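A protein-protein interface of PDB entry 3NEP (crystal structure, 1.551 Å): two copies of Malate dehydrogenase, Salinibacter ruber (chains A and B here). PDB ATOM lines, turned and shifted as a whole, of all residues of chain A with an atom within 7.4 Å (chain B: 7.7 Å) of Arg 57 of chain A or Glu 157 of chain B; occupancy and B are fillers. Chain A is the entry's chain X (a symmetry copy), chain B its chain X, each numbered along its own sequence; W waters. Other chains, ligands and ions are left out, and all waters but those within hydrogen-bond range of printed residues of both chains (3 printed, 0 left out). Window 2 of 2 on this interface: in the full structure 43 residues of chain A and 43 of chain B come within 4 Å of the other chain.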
ATOM      1  N   VAL A   3      32.003  13.943 -23.580  1.00  0.00           N
ATOM      2  CA  VAL A   3      32.734  12.979 -24.379  1.00  0.00           C
ATOM      3  C   VAL A   3      32.907  13.544 -25.767  1.00  0.00           C
ATOM      4  O   VAL A   3      31.972  14.090 -26.353  1.00  0.00           O
ATOM      5  CB  VAL A   3      31.960  11.632 -24.464  1.00  0.00           C
ATOM      6  CG1 VAL A   3      32.603  10.721 -25.488  1.00  0.00           C
ATOM      7  CG2 VAL A   3      31.844  10.937 -23.068  1.00  0.00           C
ATOM      8  N   ALA A  20      25.606   8.101 -26.193  1.00  0.00           N
ATOM      9  CA  ALA A  20      24.446   8.946 -25.963  1.00  0.00           C
ATOM     10  C   ALA A  20      23.272   8.109 -25.435  1.00  0.00           C
ATOM     11  O   ALA A  20      22.608   8.505 -24.498  1.00  0.00           O
ATOM     12  CB  ALA A  20      24.039   9.662 -27.236  1.00  0.00           C
ATOM     13  N   ASP A  23      22.961   7.436 -21.714  1.00  0.00           N
ATOM     14  CA  ASP A  23      22.385   8.539 -20.936  1.00  0.00           C
ATOM     15  C   ASP A  23      23.155   8.782 -19.645  1.00  0.00           C
ATOM     16  O   ASP A  23      22.560   9.078 -18.621  1.00  0.00           O
ATOM     17  CB  ASP A  23      20.893   8.252 -20.643  1.00  0.00           C
ATOM     18  CG  ASP A  23      20.097   9.506 -20.363  1.00  0.00           C
ATOM     19  OD1 ASP A  23      20.501  10.579 -20.864  1.00  0.00           O
ATOM     20  OD2 ASP A  23      19.065   9.407 -19.637  1.00  0.00           O
ATOM     21  N   ALA A  25      26.593  10.499 -19.938  1.00  0.00           N
ATOM     22  CA  ALA A  25      27.274  11.768 -20.244  1.00  0.00           C
ATOM     23  C   ALA A  25      26.224  12.883 -20.495  1.00  0.00           C
ATOM     24  O   ALA A  25      25.122  12.624 -20.961  1.00  0.00           O
ATOM     25  CB  ALA A  25      28.151  11.613 -21.440  1.00  0.00           C
ATOM     26  N   LYS A  26      26.577  14.119 -20.168  1.00  0.00           N
ATOM     27  CA  LYS A  26      25.731  15.277 -20.426  1.00  0.00           C
ATOM     28  C   LYS A  26      25.755  15.627 -21.918  1.00  0.00           C
ATOM     29  O   LYS A  26      24.754  16.023 -22.531  1.00  0.00           O
ATOM     30  CB  LYS A  26      26.257  16.447 -19.568  1.00  0.00           C
ATOM     31  CG  LYS A  26      25.515  17.719 -19.715  1.00  0.00           C
ATOM     32  CD  LYS A  26      24.146  17.698 -18.994  1.00  0.00           C
ATOM     33  CE  LYS A  26      23.424  19.027 -19.269  1.00  0.00           C
ATOM     34  NZ  LYS A  26      22.055  19.065 -18.687  1.00  0.00           N
ATOM     35  N   GLU A  27      26.922  15.444 -22.515  1.00  0.00           N
ATOM     36  CA  GLU A  27      27.111  15.762 -23.915  1.00  0.00           C
ATOM     37  C   GLU A  27      28.146  14.894 -24.594  1.00  0.00           C
ATOM     38  O   GLU A  27      29.146  14.465 -23.991  1.00  0.00           O
ATOM     39  CB  GLU A  27      27.493  17.235 -24.114  1.00  0.00           C
ATOM     40  CG  GLU A  27      28.261  17.468 -25.419  1.00  0.00           C
ATOM     41  CD  GLU A  27      27.649  18.539 -26.305  1.00  0.00           C
ATOM     42  OE1 GLU A  27      28.025  19.726 -26.191  1.00  0.00           O
ATOM     43  OE2 GLU A  27      26.823  18.180 -27.147  1.00  0.00           O
ATOM     44  N   VAL A  28      27.861  14.604 -25.853  1.00  0.00           N
ATOM     45  CA  VAL A  28      28.757  13.918 -26.757  1.00  0.00           C
ATOM     46  C   VAL A  28      28.951  14.791 -27.994  1.00  0.00           C
ATOM     47  O   VAL A  28      27.988  15.239 -28.598  1.00  0.00           O
ATOM     48  CB  VAL A  28      28.198  12.549 -27.194  1.00  0.00           C
ATOM     49  CG1 VAL A  28      29.127  11.908 -28.209  1.00  0.00           C
ATOM     50  CG2 VAL A  28      28.020  11.657 -26.000  1.00  0.00           C
ATOM     51  N   VAL A  29      30.202  15.049 -28.347  1.00  0.00           N
ATOM     52  CA  VAL A  29      30.550  15.906 -29.468  1.00  0.00           C
ATOM     53  C   VAL A  29      31.322  15.112 -30.523  1.00  0.00           C
ATOM     54  O   VAL A  29      32.354  14.530 -30.230  1.00  0.00           O
ATOM     55  CB  VAL A  29      31.447  17.092 -29.016  1.00  0.00           C
ATOM     56  CG1 VAL A  29      31.734  17.998 -30.206  1.00  0.00           C
ATOM     57  CG2 VAL A  29      30.802  17.847 -27.855  1.00  0.00           C
ATOM     58  N   ALA A  42      24.616  14.281 -36.028  1.00  0.00           N
ATOM     59  CA  ALA A  42      24.275  14.692 -34.696  1.00  0.00           C
ATOM     60  C   ALA A  42      22.826  15.130 -34.616  1.00  0.00           C
ATOM     61  O   ALA A  42      22.129  14.770 -33.668  1.00  0.00           O
ATOM     62  CB  ALA A  42      25.208  15.803 -34.199  1.00  0.00           C
ATOM     63  N   LEU A  43      22.374  15.857 -35.639  1.00  0.00           N
ATOM     64  CA  LEU A  43      20.981  16.289 -35.699  1.00  0.00           C
ATOM     65  C   LEU A  43      20.029  15.071 -35.761  1.00  0.00           C
ATOM     66  O   LEU A  43      19.005  15.025 -35.091  1.00  0.00           O
ATOM     67  CB  LEU A  43      20.773  17.230 -36.865  1.00  0.00           C
ATOM     68  CG  LEU A  43      19.372  17.798 -37.080  1.00  0.00           C
ATOM     69  CD1 LEU A  43      18.842  18.413 -35.812  1.00  0.00           C
ATOM     70  CD2 LEU A  43      19.492  18.828 -38.143  1.00  0.00           C
ATOM     71  N   ARG A  46      19.929  13.601 -32.352  1.00  0.00           N
ATOM     72  CA  ARG A  46      19.155  14.419 -31.402  1.00  0.00           C
ATOM     73  C   ARG A  46      17.664  14.179 -31.661  1.00  0.00           C
ATOM     74  O   ARG A  46      16.876  14.131 -30.724  1.00  0.00           O
ATOM     75  CB  ARG A  46      19.453  15.910 -31.605  1.00  0.00           C
ATOM     76  CG  ARG A  46      20.830  16.329 -31.161  1.00  0.00           C
ATOM     77  CD  ARG A  46      20.920  17.835 -30.886  1.00  0.00           C
ATOM     78  NE  ARG A  46      20.795  18.670 -32.058  1.00  0.00           N
ATOM     79  CZ  ARG A  46      21.778  18.928 -32.913  1.00  0.00           C
ATOM     80  NH1 ARG A  46      21.558  19.734 -33.942  1.00  0.00           N
ATOM     81  NH2 ARG A  46      22.967  18.369 -32.749  1.00  0.00           N
ATOM     82  N   SER A  49      16.413  11.192 -29.969  1.00  0.00           N
ATOM     83  CA  SER A  49      16.500  11.173 -28.518  1.00  0.00           C
ATOM     84  C   SER A  49      15.173  11.010 -27.777  1.00  0.00           C
ATOM     85  O   SER A  49      15.146  10.306 -26.794  1.00  0.00           O
ATOM     86  CB  SER A  49      17.313  12.383 -28.012  1.00  0.00           C
ATOM     87  OG  SER A  49      16.629  13.627 -28.189  1.00  0.00           O
ATOM     88  N   PHE A  54      16.764   9.336 -24.278  1.00  0.00           N
ATOM     89  CA  PHE A  54      18.013   9.815 -23.664  1.00  0.00           C
ATOM     90  C   PHE A  54      18.105  11.328 -23.723  1.00  0.00           C
ATOM     91  O   PHE A  54      17.570  11.960 -24.634  1.00  0.00           O
ATOM     92  CB  PHE A  54      19.261   9.137 -24.273  1.00  0.00           C
ATOM     93  CG  PHE A  54      19.504   9.429 -25.749  1.00  0.00           C
ATOM     94  CD1 PHE A  54      20.153  10.589 -26.157  1.00  0.00           C
ATOM     95  CD2 PHE A  54      19.149   8.492 -26.718  1.00  0.00           C
ATOM     96  CE1 PHE A  54      20.388  10.836 -27.497  1.00  0.00           C
ATOM     97  CE2 PHE A  54      19.363   8.728 -28.032  1.00  0.00           C
ATOM     98  CZ  PHE A  54      20.003   9.906 -28.436  1.00  0.00           C
ATOM     99  N   ASP A  55      18.729  11.908 -22.703  1.00  0.00           N
ATOM    100  CA  ASP A  55      18.915  13.349 -22.622  1.00  0.00           C
ATOM    101  C   ASP A  55      20.322  13.820 -22.928  1.00  0.00           C
ATOM    102  O   ASP A  55      20.544  15.006 -23.019  1.00  0.00           O
ATOM    103  CB  ASP A  55      18.458  13.864 -21.251  1.00  0.00           C
ATOM    104  CG  ASP A  55      16.921  13.991 -21.185  1.00  0.00           C
ATOM    105  OD1 ASP A  55      16.340  14.605 -22.125  1.00  0.00           O
ATOM    106  OD2 ASP A  55      16.319  13.464 -20.237  1.00  0.00           O
ATOM    107  N   THR A  56      21.250  12.903 -23.131  1.00  0.00           N
ATOM    108  CA  THR A  56      22.585  13.279 -23.577  1.00  0.00           C
ATOM    109  C   THR A  56      22.476  14.130 -24.825  1.00  0.00           C
ATOM    110  O   THR A  56      21.811  13.751 -25.788  1.00  0.00           O
ATOM    111  CB  THR A  56      23.385  12.041 -23.959  1.00  0.00           C
ATOM    112  OG1 THR A  56      23.425  11.156 -22.842  1.00  0.00           O
ATOM    113  CG2 THR A  56      24.806  12.399 -24.411  1.00  0.00           C
ATOM    114  N   ARG A  57      23.103  15.287 -24.808  1.00  0.00           N
ATOM    115  CA  ARG A  57      23.087  16.166 -25.981  1.00  0.00           C
ATOM    116  C   ARG A  57      24.172  15.746 -26.969  1.00  0.00           C
ATOM    117  O   ARG A  57      25.335  15.657 -26.622  1.00  0.00           O
ATOM    118  CB  ARG A  57      23.266  17.653 -25.603  1.00  0.00           C
ATOM    119  CG  ARG A  57      23.270  18.532 -26.872  1.00  0.00           C
ATOM    120  CD  ARG A  57      23.437  20.027 -26.683  1.00  0.00           C
ATOM    121  NE  ARG A  57      22.640  20.725 -27.711  1.00  0.00           N
ATOM    122  CZ  ARG A  57      22.995  20.897 -28.988  1.00  0.00           C
ATOM    123  NH1 ARG A  57      24.172  20.475 -29.439  1.00  0.00           N
ATOM    124  NH2 ARG A  57      22.170  21.511 -29.821  1.00  0.00           N
ATOM    125  N   VAL A  58      23.788  15.452 -28.194  1.00  0.00           N
ATOM    126  CA  VAL A  58      24.769  15.128 -29.233  1.00  0.00           C
ATOM    127  C   VAL A  58      24.959  16.328 -30.157  1.00  0.00           C
ATOM    128  O   VAL A  58      24.001  16.874 -30.721  1.00  0.00           O
ATOM    129  CB  VAL A  58      24.330  13.915 -30.066  1.00  0.00           C
ATOM    130  CG1 VAL A  58      25.436  13.558 -31.079  1.00  0.00           C
ATOM    131  CG2 VAL A  58      24.019  12.736 -29.157  1.00  0.00           C
ATOM    132  N   THR A  59      26.214  16.716 -30.324  1.00  0.00           N
ATOM    133  CA  THR A  59      26.651  17.847 -31.125  1.00  0.00           C
ATOM    134  C   THR A  59      27.588  17.382 -32.213  1.00  0.00           C
ATOM    135  O   THR A  59      28.330  16.416 -32.018  1.00  0.00           O
ATOM    136  CB  THR A  59      27.440  18.835 -30.220  1.00  0.00           C
ATOM    137  OG1 THR A  59      26.534  19.336 -29.251  1.00  0.00           O
ATOM    138  CG2 THR A  59      27.953  19.993 -31.004  1.00  0.00           C
ATOM    139  N   GLY A  60      27.565  18.028 -33.361  1.00  0.00           N
ATOM    140  CA  GLY A  60      28.539  17.738 -34.402  1.00  0.00           C
ATOM    141  C   GLY A  60      29.198  19.027 -34.845  1.00  0.00           C
ATOM    142  O   GLY A  60      28.562  20.068 -34.893  1.00  0.00           O
ATOM    143  N   PHE B 151       9.705  16.920 -33.571  1.00  0.00           N
ATOM    144  CA  PHE B 151       9.031  18.044 -32.927  1.00  0.00           C
ATOM    145  C   PHE B 151       9.345  18.074 -31.425  1.00  0.00           C
ATOM    146  O   PHE B 151       9.682  19.109 -30.893  1.00  0.00           O
ATOM    147  CB  PHE B 151       7.542  17.900 -33.169  1.00  0.00           C
ATOM    148  CG  PHE B 151       6.730  19.103 -32.837  1.00  0.00           C
ATOM    149  CD1 PHE B 151       6.929  20.252 -33.494  1.00  0.00           C
ATOM    150  CD2 PHE B 151       5.726  19.033 -31.907  1.00  0.00           C
ATOM    151  CE1 PHE B 151       6.154  21.388 -33.222  1.00  0.00           C
ATOM    152  CE2 PHE B 151       4.938  20.172 -31.625  1.00  0.00           C
ATOM    153  CZ  PHE B 151       5.183  21.344 -32.289  1.00  0.00           C
ATOM    154  N   ARG B 152       9.283  16.919 -30.751  1.00  0.00           N
ATOM    155  CA  ARG B 152       9.576  16.870 -29.343  1.00  0.00           C
ATOM    156  C   ARG B 152      11.028  17.286 -29.087  1.00  0.00           C
ATOM    157  O   ARG B 152      11.318  17.965 -28.110  1.00  0.00           O
ATOM    158  CB  ARG B 152       9.368  15.469 -28.814  1.00  0.00           C
ATOM    159  CG  ARG B 152       7.906  15.006 -28.761  1.00  0.00           C
ATOM    160  CD  ARG B 152       7.800  13.490 -28.645  1.00  0.00           C
ATOM    161  NE  ARG B 152       8.257  13.089 -27.326  1.00  0.00           N
ATOM    162  CZ  ARG B 152       8.620  11.872 -26.979  1.00  0.00           C
ATOM    163  NH1 ARG B 152       8.540  10.892 -27.842  1.00  0.00           N
ATOM    164  NH2 ARG B 152       9.025  11.652 -25.731  1.00  0.00           N
ATOM    165  N   SER B 153      11.954  16.849 -29.931  1.00  0.00           N
ATOM    166  CA  SER B 153      13.334  17.175 -29.712  1.00  0.00           C
ATOM    167  C   SER B 153      13.579  18.668 -29.813  1.00  0.00           C
ATOM    168  O   SER B 153      14.340  19.221 -29.005  1.00  0.00           O
ATOM    169  CB  SER B 153      14.255  16.381 -30.642  1.00  0.00           C
ATOM    170  OG  SER B 153      14.319  16.918 -31.923  1.00  0.00           O
ATOM    171  N   PHE B 154      12.889  19.323 -30.750  1.00  0.00           N
ATOM    172  CA  PHE B 154      13.036  20.760 -30.928  1.00  0.00           C
ATOM    173  C   PHE B 154      12.439  21.523 -29.739  1.00  0.00           C
ATOM    174  O   PHE B 154      13.015  22.509 -29.282  1.00  0.00           O
ATOM    175  CB  PHE B 154      12.367  21.222 -32.229  1.00  0.00           C
ATOM    176  CG  PHE B 154      12.918  20.590 -33.472  1.00  0.00           C
ATOM    177  CD1 PHE B 154      12.104  20.331 -34.560  1.00  0.00           C
ATOM    178  CD2 PHE B 154      14.250  20.236 -33.554  1.00  0.00           C
ATOM    179  CE1 PHE B 154      12.591  19.777 -35.690  1.00  0.00           C
ATOM    180  CE2 PHE B 154      14.728  19.636 -34.715  1.00  0.00           C
ATOM    181  CZ  PHE B 154      13.905  19.414 -35.774  1.00  0.00           C
ATOM    182  N   ILE B 155      11.292  21.054 -29.234  1.00  0.00           N
ATOM    183  CA  ILE B 155      10.643  21.669 -28.082  1.00  0.00           C
ATOM    184  C   ILE B 155      11.540  21.513 -26.851  1.00  0.00           C
ATOM    185  O   ILE B 155      11.760  22.454 -26.103  1.00  0.00           O
ATOM    186  CB  ILE B 155       9.239  21.029 -27.818  1.00  0.00           C
ATOM    187  CG1 ILE B 155       8.273  21.322 -28.982  1.00  0.00           C
ATOM    188  CG2 ILE B 155       8.664  21.518 -26.514  1.00  0.00           C
ATOM    189  CD1 ILE B 155       7.754  22.716 -29.029  1.00  0.00           C
ATOM    190  N   ALA B 156      12.070  20.310 -26.642  1.00  0.00           N
ATOM    191  CA  ALA B 156      12.886  20.056 -25.470  1.00  0.00           C
ATOM    192  C   ALA B 156      14.143  20.931 -25.502  1.00  0.00           C
ATOM    193  O   ALA B 156      14.555  21.460 -24.478  1.00  0.00           O
ATOM    194  CB  ALA B 156      13.242  18.627 -25.415  1.00  0.00           C
ATOM    195  N   GLU B 157      14.739  21.077 -26.677  1.00  0.00           N
ATOM    196  CA  GLU B 157      15.907  21.941 -26.878  1.00  0.00           C
ATOM    197  C   GLU B 157      15.581  23.414 -26.583  1.00  0.00           C
ATOM    198  O   GLU B 157      16.361  24.128 -25.943  1.00  0.00           O
ATOM    199  CB  GLU B 157      16.395  21.788 -28.320  1.00  0.00           C
ATOM    200  CG  GLU B 157      17.676  22.520 -28.642  1.00  0.00           C
ATOM    201  CD  GLU B 157      18.132  22.308 -30.100  1.00  0.00           C
ATOM    202  OE1 GLU B 157      17.357  22.599 -31.054  1.00  0.00           O
ATOM    203  OE2 GLU B 157      19.283  21.860 -30.283  1.00  0.00           O
ATOM    204  N   GLU B 158      14.418  23.862 -27.044  1.00  0.00           N
ATOM    205  CA  GLU B 158      13.987  25.251 -26.864  1.00  0.00           C
ATOM    206  C   GLU B 158      13.753  25.595 -25.400  1.00  0.00           C
ATOM    207  O   GLU B 158      14.129  26.670 -24.959  1.00  0.00           O
ATOM    208  CB  GLU B 158      12.708  25.522 -27.665  1.00  0.00           C
ATOM    209  CG  GLU B 158      12.119  26.988 -27.487  1.00  0.00           C
ATOM    210  CD  GLU B 158      12.918  28.068 -28.120  1.00  0.00           C
ATOM    211  OE1 GLU B 158      13.761  27.760 -28.983  1.00  0.00           O
ATOM    212  OE2 GLU B 158      12.690  29.243 -27.766  1.00  0.00           O
ATOM    213  N   LEU B 159      13.164  24.678 -24.640  1.00  0.00           N
ATOM    214  CA  LEU B 159      12.850  24.927 -23.242  1.00  0.00           C
ATOM    215  C   LEU B 159      13.945  24.479 -22.280  1.00  0.00           C
ATOM    216  O   LEU B 159      13.886  24.801 -21.091  1.00  0.00           O
ATOM    217  CB  LEU B 159      11.537  24.239 -22.845  1.00  0.00           C
ATOM    218  CG  LEU B 159      10.304  24.737 -23.612  1.00  0.00           C
ATOM    219  CD1 LEU B 159       9.165  23.738 -23.441  1.00  0.00           C
ATOM    220  CD2 LEU B 159       9.911  26.099 -23.121  1.00  0.00           C
ATOM    221  N   ASP B 160      14.922  23.723 -22.795  1.00  0.00           N
ATOM    222  CA  ASP B 160      15.922  23.045 -21.973  1.00  0.00           C
ATOM    223  C   ASP B 160      15.231  22.167 -20.921  1.00  0.00           C
ATOM    224  O   ASP B 160      15.411  22.340 -19.707  1.00  0.00           O
ATOM    225  CB  ASP B 160      16.925  24.014 -21.315  1.00  0.00           C
ATOM    226  CG  ASP B 160      18.118  23.279 -20.730  1.00  0.00           C
ATOM    227  OD1 ASP B 160      18.383  22.164 -21.218  1.00  0.00           O
ATOM    228  OD2 ASP B 160      18.768  23.776 -19.784  1.00  0.00           O
ATOM    229  N   VAL B 161      14.414  21.233 -21.414  1.00  0.00           N
ATOM    230  CA  VAL B 161      13.728  20.245 -20.574  1.00  0.00           C
ATOM    231  C   VAL B 161      14.010  18.851 -21.088  1.00  0.00           C
ATOM    232  O   VAL B 161      14.348  18.665 -22.258  1.00  0.00           O
ATOM    233  CB  VAL B 161      12.184  20.458 -20.568  1.00  0.00           C
ATOM    234  CG1 VAL B 161      11.872  21.791 -19.896  1.00  0.00           C
ATOM    235  CG2 VAL B 161      11.662  20.424 -21.998  1.00  0.00           C
ATOM    236  N   SER B 162      13.800  17.862 -20.241  1.00  0.00           N
ATOM    237  CA  SER B 162      13.991  16.465 -20.650  1.00  0.00           C
ATOM    238  C   SER B 162      13.058  16.070 -21.789  1.00  0.00           C
ATOM    239  O   SER B 162      11.869  16.374 -21.779  1.00  0.00           O
ATOM    240  CB  SER B 162      13.764  15.530 -19.476  1.00  0.00           C
ATOM    241  OG  SER B 162      13.881  14.178 -19.916  1.00  0.00           O
ATOM    242  N   VAL B 163      13.581  15.353 -22.760  1.00  0.00           N
ATOM    243  CA  VAL B 163      12.759  14.812 -23.825  1.00  0.00           C
ATOM    244  C   VAL B 163      11.698  13.853 -23.269  1.00  0.00           C
ATOM    245  O   VAL B 163      10.648  13.619 -23.898  1.00  0.00           O
ATOM    246  CB  VAL B 163      13.596  14.055 -24.886  1.00  0.00           C
ATOM    247  CG1 VAL B 163      14.633  14.953 -25.502  1.00  0.00           C
ATOM    248  CG2 VAL B 163      14.261  12.837 -24.281  1.00  0.00           C
ATOM    249  N   VAL B 166       8.303  15.670 -22.795  1.00  0.00           N
ATOM    250  CA  VAL B 166       7.650  16.342 -23.910  1.00  0.00           C
ATOM    251  C   VAL B 166       6.874  15.314 -24.739  1.00  0.00           C
ATOM    252  O   VAL B 166       7.414  14.271 -25.118  1.00  0.00           O
ATOM    253  CB  VAL B 166       8.665  17.096 -24.785  1.00  0.00           C
ATOM    254  CG1 VAL B 166       7.965  17.807 -25.919  1.00  0.00           C
ATOM    255  CG2 VAL B 166       9.440  18.067 -23.979  1.00  0.00           C
ATOM    256  N   ILE B 196       5.732  28.552 -24.782  1.00  0.00           N
ATOM    257  CA  ILE B 196       6.419  29.066 -25.949  1.00  0.00           C
ATOM    258  C   ILE B 196       5.444  29.961 -26.697  1.00  0.00           C
ATOM    259  O   ILE B 196       4.271  29.615 -26.817  1.00  0.00           O
ATOM    260  CB  ILE B 196       6.877  27.903 -26.849  1.00  0.00           C
ATOM    261  CG1 ILE B 196       7.751  26.928 -26.033  1.00  0.00           C
ATOM    262  CG2 ILE B 196       7.658  28.398 -28.030  1.00  0.00           C
ATOM    263  CD1 ILE B 196       8.375  25.791 -26.912  1.00  0.00           C
ATOM    264  N   ARG B 200       7.487  31.466 -32.172  1.00  0.00           N
ATOM    265  CA  ARG B 200       8.486  30.408 -31.965  1.00  0.00           C
ATOM    266  C   ARG B 200       7.911  29.017 -32.196  1.00  0.00           C
ATOM    267  O   ARG B 200       8.593  28.141 -32.738  1.00  0.00           O
ATOM    268  CB  ARG B 200       9.072  30.547 -30.567  1.00  0.00           C
ATOM    269  CG  ARG B 200      10.225  29.661 -30.286  1.00  0.00           C
ATOM    270  CD  ARG B 200      11.364  29.903 -31.287  1.00  0.00           C
ATOM    271  NE  ARG B 200      12.399  28.933 -30.993  1.00  0.00           N
ATOM    272  CZ  ARG B 200      13.040  28.225 -31.896  1.00  0.00           C
ATOM    273  NH1 ARG B 200      13.889  27.278 -31.494  1.00  0.00           N
ATOM    274  NH2 ARG B 200      12.835  28.452 -33.178  1.00  0.00           N
ATOM    275  N   ILE B 204       9.166  26.236 -35.062  1.00  0.00           N
ATOM    276  CA  ILE B 204       9.452  24.828 -34.775  1.00  0.00           C
ATOM    277  C   ILE B 204       8.609  23.908 -35.680  1.00  0.00           C
ATOM    278  O   ILE B 204       9.056  22.870 -36.142  1.00  0.00           O
ATOM    279  CB  ILE B 204       9.243  24.546 -33.288  1.00  0.00           C
ATOM    280  CG1 ILE B 204      10.337  25.255 -32.482  1.00  0.00           C
ATOM    281  CG2 ILE B 204       9.276  23.036 -33.019  1.00  0.00           C
ATOM    282  CD1 ILE B 204      10.121  25.282 -30.981  1.00  0.00           C
ATOM    283  N   ARG B 207      10.244  23.873 -39.016  1.00  0.00           N
ATOM    284  CA  ARG B 207      11.447  23.040 -38.987  1.00  0.00           C
ATOM    285  C   ARG B 207      11.094  21.556 -39.025  1.00  0.00           C
ATOM    286  O   ARG B 207      11.764  20.760 -39.680  1.00  0.00           O
ATOM    287  CB  ARG B 207      12.275  23.348 -37.758  1.00  0.00           C
ATOM    288  CG  ARG B 207      13.646  22.696 -37.817  1.00  0.00           C
ATOM    289  CD  ARG B 207      14.421  22.902 -36.571  1.00  0.00           C
ATOM    290  NE  ARG B 207      15.755  22.367 -36.776  1.00  0.00           N
ATOM    291  CZ  ARG B 207      16.709  22.368 -35.869  1.00  0.00           C
ATOM    292  NH1 ARG B 207      16.490  22.841 -34.665  1.00  0.00           N
ATOM    293  NH2 ARG B 207      17.892  21.874 -36.185  1.00  0.00           N
HETATM  294  O   HOH W   1      20.104  22.477 -34.299  1.00  0.00           O
HETATM  295  O   HOH W   2      18.464  20.366 -32.905  1.00  0.00           O
HETATM  296  O   HOH W   3      20.964  21.474 -20.036  1.00  0.00           O
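OE2 of Glu 157 of chain B lies within salt-bridge range of NE of Arg 46 of chain A (3.95 Å). OE2 of Glu 157 of chain B is in salt-bridge range of NH2 of Arg 57 of chain A, at 2.9 Å. The side-chain hydroxyl (OG) of Ser 162 of chain B sits at hydrogen-bond distance from the side-chain carboxylate (OD2) of Asp 55 of chain A. N of Val 163 of chain B lies within hydrogen-bond range of OD1 of Asp 55 of chain A, 2.9 Å away.
The backbone carbonyl oxygen (O) of Val 163 of chain B sits at hydrogen-bond distance from the guanidinium group (NH2) of Arg 152 of chain B (3.1 Å). The side-chain carboxylate (OE1) of Glu 157 of chain B lies within salt-bridge range of the guanidinium group (NH1) of Arg 207 of chain B (3.7 Å). The side-chain carboxylate (OD1) of Asp 23 of chain A is in hydrogen-bond range of the backbone NH (N) of Asp 55 of chain A (2.9 Å). OG of Ser 49 of chain A lies within hydrogen-bond range of O of Arg 46 of chain A (2.6 Å). The guanidinium group (NH2) of Arg 46 of chain A lies within hydrogen-bond range of the backbone carbonyl oxygen (O) of Val 58 of chain A (2.7 Å). The guanidinium group (NH1) of Arg 57 of chain A sits at hydrogen-bond distance from the side-chain hydroxyl (OG1) of Thr 59 of chain A (2.6 Å).
Among the printed residues, pairs that only touch across the chains: Phe 54 of chain A with Val 163 of chain B (3.4 Å), Arg 46 of chain A with Ser 153 of chain B (3.5 Å), Ser 49 of chain A with Val 163 of chain B (3.6 Å) and Leu 43 of chain A with Arg 207 of chain B (3.6 Å).
Asp 23 of chain A touches none of the printed residues of chain B. Printed residues of chain B within 4 Å of Arg 46 of chain A: Ser 153 and Glu 157. Printed residues of chain B within 4 Å of Asp 55 of chain A: Ser 162 (2.6 Å) and Val 163 (2.9 Å). Arg 57 of chain A touches one residue of chain B. Phe 151 of chain B touches none of the printed residues of chain A. Printed residues of chain A within 4 Å of Ser 153 of chain B: Arg 46. No residue of chain A comes within 4 Å of Ala 156 of chain B. Of chain A, only Arg 46 and Arg 57 come within 4 Å of Glu 157 of chain B. Of the printed residues of chain A, Ser 162 of chain B touches Asp 55 (2.6 Å). The nearest printed residue of chain B that does not touch Leu 43 of chain A is Phe 154 of chain B (4.4 Å).
Printed residues of chain B that touch a printed residue of chain A: Ser 153, Glu 157, Ser 162, Val 163 and Arg 207. Hydrophobic or aromatic side chains of chain B that line the printed part of chain A: Val 163. Along chain B the printed residues that touch a printed residue of chain A span positions 153 to 207. Of the 19 printed residues of chain A, 6 touch a printed residue of chain B. Along chain A the printed residues that touch a printed residue of chain B span positions 43 to 57.
No position is printed for both chains.
Water W3 bridges OD1 of Asp 160 of chain B and NZ of Lys 26 of chain A. Water W1 bridges the guanidinium group (NH2) of Arg 207 of chain B (3.0 Å) and the guanidinium group (NH1) of Arg 46 of chain A (3.1 Å). Water W2 lies within hydrogen-bond range of the guanidinium group (NE) of Arg 46 of chain A (3.0 Å) and the side-chain carboxylate (OE1) of Glu 157 of chain B (3.1 Å).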
